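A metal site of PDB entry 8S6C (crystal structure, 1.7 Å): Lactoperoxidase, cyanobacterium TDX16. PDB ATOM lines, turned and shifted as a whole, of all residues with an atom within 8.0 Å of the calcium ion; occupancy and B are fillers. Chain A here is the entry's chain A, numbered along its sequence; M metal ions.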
ATOM      1  N   ARG A   4      27.546   1.860 -23.782  1.00  0.00           N
ATOM      2  CA  ARG A   4      27.321   2.845 -22.756  1.00  0.00           C
ATOM      3  C   ARG A   4      27.956   2.387 -21.429  1.00  0.00           C
ATOM      4  O   ARG A   4      27.971   1.193 -21.100  1.00  0.00           O
ATOM      5  CB  ARG A   4      25.817   2.951 -22.505  1.00  0.00           C
ATOM      6  CG  ARG A   4      24.938   3.574 -23.568  1.00  0.00           C
ATOM      7  CD  ARG A   4      23.577   3.572 -22.936  1.00  0.00           C
ATOM      8  NE  ARG A   4      22.533   4.057 -23.832  1.00  0.00           N
ATOM      9  CZ  ARG A   4      22.269   5.338 -24.127  1.00  0.00           C
ATOM     10  NH1 ARG A   4      22.943   6.326 -23.566  1.00  0.00           N
ATOM     11  NH2 ARG A   4      21.280   5.627 -24.975  1.00  0.00           N
ATOM     12  N   ILE A   6      27.524   2.151 -17.373  1.00  0.00           N
ATOM     13  CA  ILE A   6      26.334   1.947 -16.583  1.00  0.00           C
ATOM     14  C   ILE A   6      25.936   3.276 -15.923  1.00  0.00           C
ATOM     15  O   ILE A   6      24.747   3.484 -15.636  1.00  0.00           O
ATOM     16  CB  ILE A   6      26.515   0.819 -15.554  1.00  0.00           C
ATOM     17  CG1 ILE A   6      26.405  -0.551 -16.191  1.00  0.00           C
ATOM     18  CG2 ILE A   6      25.519   0.921 -14.415  1.00  0.00           C
ATOM     19  CD1 ILE A   6      24.963  -0.934 -16.524  1.00  0.00           C
ATOM     20  N   ASP A   7      26.921   4.151 -15.636  1.00  0.00           N
ATOM     21  CA  ASP A   7      26.626   5.350 -14.858  1.00  0.00           C
ATOM     22  C   ASP A   7      26.331   6.568 -15.720  1.00  0.00           C
ATOM     23  O   ASP A   7      26.070   7.649 -15.188  1.00  0.00           O
ATOM     24  CB  ASP A   7      27.711   5.679 -13.834  1.00  0.00           C
ATOM     25  CG  ASP A   7      29.086   6.000 -14.405  1.00  0.00           C
ATOM     26  OD1 ASP A   7      29.177   6.144 -15.655  1.00  0.00           O
ATOM     27  OD2 ASP A   7      30.042   6.103 -13.591  1.00  0.00           O
ATOM     28  N   GLY A   8      26.394   6.425 -17.041  1.00  0.00           N
ATOM     29  CA  GLY A   8      26.011   7.500 -17.934  1.00  0.00           C
ATOM     30  C   GLY A   8      27.151   8.472 -18.226  1.00  0.00           C
ATOM     31  O   GLY A   8      26.959   9.415 -18.992  1.00  0.00           O
ATOM     32  N   GLY A  19      24.831  13.915 -17.905  1.00  0.00           N
ATOM     33  CA  GLY A  19      23.848  12.850 -18.073  1.00  0.00           C
ATOM     34  C   GLY A  19      24.012  11.705 -17.071  1.00  0.00           C
ATOM     35  O   GLY A  19      23.164  10.811 -17.023  1.00  0.00           O
ATOM     36  N   THR A  21      25.017   9.686 -13.251  1.00  0.00           N
ATOM     37  CA  THR A  21      24.446   9.671 -11.912  1.00  0.00           C
ATOM     38  C   THR A  21      25.043  10.799 -11.074  1.00  0.00           C
ATOM     39  O   THR A  21      26.225  11.125 -11.210  1.00  0.00           O
ATOM     40  CB  THR A  21      24.693   8.312 -11.254  1.00  0.00           C
ATOM     41  OG1 THR A  21      26.115   8.201 -11.317  1.00  0.00           O
ATOM     42  CG2 THR A  21      24.113   7.175 -12.052  1.00  0.00           C
ATOM     43  N   LEU A  79       9.272   4.941 -17.692  1.00  0.00           N
ATOM     44  CA  LEU A  79      10.219   5.813 -18.366  1.00  0.00           C
ATOM     45  C   LEU A  79      10.748   6.882 -17.401  1.00  0.00           C
ATOM     46  O   LEU A  79      11.932   7.160 -17.383  1.00  0.00           O
ATOM     47  CB  LEU A  79       9.504   6.379 -19.589  1.00  0.00           C
ATOM     48  CG  LEU A  79      10.267   7.497 -20.304  1.00  0.00           C
ATOM     49  CD1 LEU A  79      11.605   7.028 -20.835  1.00  0.00           C
ATOM     50  CD2 LEU A  79       9.449   8.142 -21.415  1.00  0.00           C
ATOM     51  N   ASP A  80       9.884   7.405 -16.525  1.00  0.00           N
ATOM     52  CA  ASP A  80      10.316   8.301 -15.467  1.00  0.00           C
ATOM     53  C   ASP A  80      11.461   7.680 -14.671  1.00  0.00           C
ATOM     54  O   ASP A  80      12.440   8.346 -14.344  1.00  0.00           O
ATOM     55  CB  ASP A  80       9.189   8.645 -14.512  1.00  0.00           C
ATOM     56  CG  ASP A  80       9.587   9.708 -13.497  1.00  0.00           C
ATOM     57  OD1 ASP A  80       9.848  10.825 -13.903  1.00  0.00           O
ATOM     58  OD2 ASP A  80       9.756   9.375 -12.328  1.00  0.00           O
ATOM     59  N   HIS A  81      11.339   6.374 -14.406  1.00  0.00           N
ATOM     60  CA  HIS A  81      12.297   5.656 -13.591  1.00  0.00           C
ATOM     61  C   HIS A  81      13.557   5.289 -14.368  1.00  0.00           C
ATOM     62  O   HIS A  81      14.480   4.733 -13.783  1.00  0.00           O
ATOM     63  CB  HIS A  81      11.619   4.468 -12.895  1.00  0.00           C
ATOM     64  CG  HIS A  81      10.587   4.894 -11.921  1.00  0.00           C
ATOM     65  ND1 HIS A  81       9.878   4.022 -11.119  1.00  0.00           N
ATOM     66  CD2 HIS A  81      10.085   6.121 -11.664  1.00  0.00           C
ATOM     67  CE1 HIS A  81       9.031   4.723 -10.382  1.00  0.00           C
ATOM     68  NE2 HIS A  81       9.128   5.990 -10.709  1.00  0.00           N
ATOM     69  N   ASP A  82      13.615   5.686 -15.657  1.00  0.00           N
ATOM     70  CA  ASP A  82      14.822   5.708 -16.474  1.00  0.00           C
ATOM     71  C   ASP A  82      15.432   7.115 -16.461  1.00  0.00           C
ATOM     72  O   ASP A  82      16.627   7.308 -16.677  1.00  0.00           O
ATOM     73  CB  ASP A  82      14.481   5.208 -17.882  1.00  0.00           C
ATOM     74  CG  ASP A  82      15.623   4.739 -18.772  1.00  0.00           C
ATOM     75  OD1 ASP A  82      16.795   4.951 -18.425  1.00  0.00           O
ATOM     76  OD2 ASP A  82      15.328   4.142 -19.843  1.00  0.00           O
ATOM     77  N   LEU A  83      14.615   8.141 -16.204  1.00  0.00           N
ATOM     78  CA  LEU A  83      15.065   9.501 -16.404  1.00  0.00           C
ATOM     79  C   LEU A  83      15.640  10.127 -15.133  1.00  0.00           C
ATOM     80  O   LEU A  83      16.736  10.706 -15.181  1.00  0.00           O
ATOM     81  CB  LEU A  83      13.900  10.324 -16.938  1.00  0.00           C
ATOM     82  CG  LEU A  83      13.406   9.966 -18.338  1.00  0.00           C
ATOM     83  CD1 LEU A  83      12.172  10.783 -18.670  1.00  0.00           C
ATOM     84  CD2 LEU A  83      14.454  10.177 -19.399  1.00  0.00           C
ATOM     85  N   ASP A  84      14.889  10.097 -14.026  1.00  0.00           N
ATOM     86  CA  ASP A  84      15.272  10.856 -12.852  1.00  0.00           C
ATOM     87  C   ASP A  84      14.836  10.165 -11.558  1.00  0.00           C
ATOM     88  O   ASP A  84      13.796   9.507 -11.486  1.00  0.00           O
ATOM     89  CB  ASP A  84      14.683  12.254 -12.930  1.00  0.00           C
ATOM     90  CG  ASP A  84      13.182  12.268 -13.166  1.00  0.00           C
ATOM     91  OD1 ASP A  84      12.431  12.131 -12.196  1.00  0.00           O
ATOM     92  OD2 ASP A  84      12.772  12.400 -14.340  1.00  0.00           O
ATOM     93  N   ASN A 137      20.179  14.392  -9.495  1.00  0.00           N
ATOM     94  CA  ASN A 137      19.592  13.238 -10.142  1.00  0.00           C
ATOM     95  C   ASN A 137      20.481  12.029  -9.875  1.00  0.00           C
ATOM     96  O   ASN A 137      21.685  12.076 -10.166  1.00  0.00           O
ATOM     97  CB  ASN A 137      19.458  13.460 -11.644  1.00  0.00           C
ATOM     98  CG  ASN A 137      18.672  12.378 -12.340  1.00  0.00           C
ATOM     99  OD1 ASN A 137      18.152  11.463 -11.695  1.00  0.00           O
ATOM    100  ND2 ASN A 137      18.510  12.517 -13.643  1.00  0.00           N
ATOM    101  N   ILE A 139      20.027   8.837 -10.940  1.00  0.00           N
ATOM    102  CA  ILE A 139      20.093   7.818 -11.990  1.00  0.00           C
ATOM    103  C   ILE A 139      20.556   8.517 -13.254  1.00  0.00           C
ATOM    104  O   ILE A 139      20.671   9.742 -13.240  1.00  0.00           O
ATOM    105  CB  ILE A 139      18.766   7.072 -12.144  1.00  0.00           C
ATOM    106  CG1 ILE A 139      17.610   7.993 -12.537  1.00  0.00           C
ATOM    107  CG2 ILE A 139      18.458   6.308 -10.858  1.00  0.00           C
ATOM    108  CD1 ILE A 139      16.348   7.244 -12.933  1.00  0.00           C
ATOM    109  N   THR A 140      20.899   7.728 -14.293  1.00  0.00           N
ATOM    110  CA  THR A 140      21.333   8.281 -15.563  1.00  0.00           C
ATOM    111  C   THR A 140      20.164   8.988 -16.243  1.00  0.00           C
ATOM    112  O   THR A 140      19.068   8.426 -16.383  1.00  0.00           O
ATOM    113  CB  THR A 140      21.949   7.210 -16.482  1.00  0.00           C
ATOM    114  OG1 THR A 140      20.896   6.453 -17.055  1.00  0.00           O
ATOM    115  CG2 THR A 140      22.975   6.317 -15.777  1.00  0.00           C
ATOM    116  N   SER A 141      20.385  10.232 -16.673  1.00  0.00           N
ATOM    117  CA  SER A 141      19.395  11.014 -17.407  1.00  0.00           C
ATOM    118  C   SER A 141      19.033  10.356 -18.744  1.00  0.00           C
ATOM    119  O   SER A 141      17.889  10.479 -19.204  1.00  0.00           O
ATOM    120  CB  SER A 141      19.868  12.456 -17.613  1.00  0.00           C
ATOM    121  OG  SER A 141      20.006  13.142 -16.373  1.00  0.00           O
ATOM    122  N   TRP A 142      19.995   9.653 -19.355  1.00  0.00           N
ATOM    123  CA  TRP A 142      19.826   9.009 -20.647  1.00  0.00           C
ATOM    124  C   TRP A 142      18.654   8.036 -20.613  1.00  0.00           C
ATOM    125  O   TRP A 142      18.431   7.361 -19.600  1.00  0.00           O
ATOM    126  CB  TRP A 142      21.081   8.257 -21.104  1.00  0.00           C
ATOM    127  CG  TRP A 142      22.348   9.069 -21.001  1.00  0.00           C
ATOM    128  CD1 TRP A 142      23.394   8.897 -20.135  1.00  0.00           C
ATOM    129  CD2 TRP A 142      22.626  10.259 -21.755  1.00  0.00           C
ATOM    130  NE1 TRP A 142      24.328   9.870 -20.326  1.00  0.00           N
ATOM    131  CE2 TRP A 142      23.884  10.732 -21.310  1.00  0.00           C
ATOM    132  CE3 TRP A 142      21.965  10.944 -22.766  1.00  0.00           C
ATOM    133  CZ2 TRP A 142      24.459  11.883 -21.841  1.00  0.00           C
ATOM    134  CZ3 TRP A 142      22.533  12.092 -23.291  1.00  0.00           C
ATOM    135  CH2 TRP A 142      23.769  12.562 -22.823  1.00  0.00           C
ATOM    136  N   ILE A 143      17.978   7.919 -21.766  1.00  0.00           N
ATOM    137  CA  ILE A 143      17.044   6.836 -22.001  1.00  0.00           C
ATOM    138  C   ILE A 143      17.880   5.632 -22.433  1.00  0.00           C
ATOM    139  O   ILE A 143      18.128   5.411 -23.633  1.00  0.00           O
ATOM    140  CB  ILE A 143      15.955   7.221 -23.029  1.00  0.00           C
ATOM    141  CG1 ILE A 143      15.255   8.525 -22.633  1.00  0.00           C
ATOM    142  CG2 ILE A 143      14.963   6.075 -23.221  1.00  0.00           C
ATOM    143  CD1 ILE A 143      14.218   9.020 -23.623  1.00  0.00           C
ATOM    144  N   ASP A 144      18.367   4.915 -21.429  1.00  0.00           N
ATOM    145  CA  ASP A 144      19.334   3.839 -21.614  1.00  0.00           C
ATOM    146  C   ASP A 144      18.935   2.577 -20.868  1.00  0.00           C
ATOM    147  O   ASP A 144      19.765   1.698 -20.696  1.00  0.00           O
ATOM    148  CB  ASP A 144      20.708   4.278 -21.105  1.00  0.00           C
ATOM    149  CG  ASP A 144      20.723   4.711 -19.647  1.00  0.00           C
ATOM    150  OD1 ASP A 144      19.655   4.700 -18.990  1.00  0.00           O
ATOM    151  OD2 ASP A 144      21.800   5.118 -19.176  1.00  0.00           O
ATOM    152  N   ALA A 145      17.677   2.472 -20.436  1.00  0.00           N
ATOM    153  CA  ALA A 145      17.220   1.299 -19.711  1.00  0.00           C
ATOM    154  C   ALA A 145      17.973   1.123 -18.393  1.00  0.00           C
ATOM    155  O   ALA A 145      18.134  -0.020 -17.938  1.00  0.00           O
ATOM    156  CB  ALA A 145      17.300   0.033 -20.586  1.00  0.00           C
ATOM    157  N   SER A 146      18.344   2.236 -17.724  1.00  0.00           N
ATOM    158  CA  SER A 146      18.952   2.175 -16.407  1.00  0.00           C
ATOM    159  C   SER A 146      17.923   1.633 -15.411  1.00  0.00           C
ATOM    160  O   SER A 146      18.266   1.108 -14.347  1.00  0.00           O
ATOM    161  CB  SER A 146      19.520   3.508 -15.963  1.00  0.00           C
ATOM    162  OG  SER A 146      18.544   4.549 -15.944  1.00  0.00           O
ATOM    163  N   ASN A 147      16.653   1.697 -15.787  1.00  0.00           N
ATOM    164  CA  ASN A 147      15.590   1.102 -14.990  1.00  0.00           C
ATOM    165  C   ASN A 147      15.618  -0.431 -15.011  1.00  0.00           C
ATOM    166  O   ASN A 147      15.105  -1.050 -14.068  1.00  0.00           O
ATOM    167  CB  ASN A 147      14.188   1.576 -15.366  1.00  0.00           C
ATOM    168  CG  ASN A 147      13.948   1.582 -16.854  1.00  0.00           C
ATOM    169  OD1 ASN A 147      14.766   1.114 -17.637  1.00  0.00           O
ATOM    170  ND2 ASN A 147      12.812   2.129 -17.244  1.00  0.00           N
ATOM    171  N   VAL A 148      16.252  -1.016 -16.012  1.00  0.00           N
ATOM    172  CA  VAL A 148      16.461  -2.457 -16.073  1.00  0.00           C
ATOM    173  C   VAL A 148      17.838  -2.874 -15.524  1.00  0.00           C
ATOM    174  O   VAL A 148      17.947  -3.889 -14.834  1.00  0.00           O
ATOM    175  CB  VAL A 148      16.284  -2.908 -17.535  1.00  0.00           C
ATOM    176  CG1 VAL A 148      16.525  -4.405 -17.734  1.00  0.00           C
ATOM    177  CG2 VAL A 148      14.921  -2.492 -18.071  1.00  0.00           C
ATOM    178  N   GLY A 150      20.384  -0.893 -13.859  1.00  0.00           N
ATOM    179  CA  GLY A 150      21.006  -0.177 -12.764  1.00  0.00           C
ATOM    180  C   GLY A 150      21.794   1.026 -13.283  1.00  0.00           C
ATOM    181  O   GLY A 150      21.996   1.163 -14.490  1.00  0.00           O
ATOM    182  N   SER A 151      22.133   1.925 -12.345  1.00  0.00           N
ATOM    183  CA  SER A 151      22.778   3.185 -12.653  1.00  0.00           C
ATOM    184  C   SER A 151      24.162   3.224 -12.001  1.00  0.00           C
ATOM    185  O   SER A 151      24.803   4.274 -11.997  1.00  0.00           O
ATOM    186  CB  SER A 151      21.935   4.359 -12.201  1.00  0.00           C
ATOM    187  OG  SER A 151      20.785   4.562 -13.014  1.00  0.00           O
ATOM    188  N   ILE A 281      18.391  16.024 -16.604  1.00  0.00           N
ATOM    189  CA  ILE A 281      16.951  16.242 -16.619  1.00  0.00           C
ATOM    190  C   ILE A 281      16.666  17.585 -15.946  1.00  0.00           C
ATOM    191  O   ILE A 281      17.244  17.899 -14.912  1.00  0.00           O
ATOM    192  CB  ILE A 281      16.194  15.105 -15.910  1.00  0.00           C
ATOM    193  CG1 ILE A 281      16.546  13.719 -16.497  1.00  0.00           C
ATOM    194  CG2 ILE A 281      14.698  15.345 -15.937  1.00  0.00           C
ATOM    195  CD1 ILE A 281      16.212  13.571 -17.953  1.00  0.00           C
ATOM    196  N   LEU A 458      17.088  14.735 -25.142  1.00  0.00           N
ATOM    197  CA  LEU A 458      17.528  13.368 -24.875  1.00  0.00           C
ATOM    198  C   LEU A 458      17.662  12.591 -26.188  1.00  0.00           C
ATOM    199  O   LEU A 458      18.338  11.560 -26.239  1.00  0.00           O
ATOM    200  CB  LEU A 458      16.598  12.637 -23.921  1.00  0.00           C
ATOM    201  CG  LEU A 458      16.616  13.177 -22.490  1.00  0.00           C
ATOM    202  CD1 LEU A 458      15.479  12.615 -21.687  1.00  0.00           C
ATOM    203  CD2 LEU A 458      17.935  12.861 -21.831  1.00  0.00           C
HETATM  204 CA    CA M   1      18.592   6.347 -17.528  1.00  0.00          CA
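Five residues have an atom within 4 Å of the calcium ion: Asp 82, Thr 140, Trp 142, Asp 144 and Ser 146.
The nearest printed residue that does not touch the calcium ion is Ser 141 (4.2 Å).
NE1 of Trp 142 sits at hydrogen-bond distance from O of Gly 8 (3.0 Å).
The side-chain carboxylate of Asp 82 lies within hydrogen-bond range of the backbone NH of Ala 145, at 2.9 Å.
The side-chain hydroxyl (OG) of Ser 151 is in hydrogen-bond range of the backbone NH (N) of Thr 140.
The calcium ion is bound by the backbone carbonyl oxygen (O) of Trp 142, the backbone carbonyl oxygen (O) of Asp 82, the side-chain hydroxyl (OG1) of Thr 140, the side-chain hydroxyl (OG) of Ser 146, the backbone carbonyl oxygen (O) of Thr 140, the side-chain carboxylate (OD1) of Asp 144 and the side-chain carboxylate (OD1) of Asp 82.
The calcium ion has seven donor atoms within binding distance.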
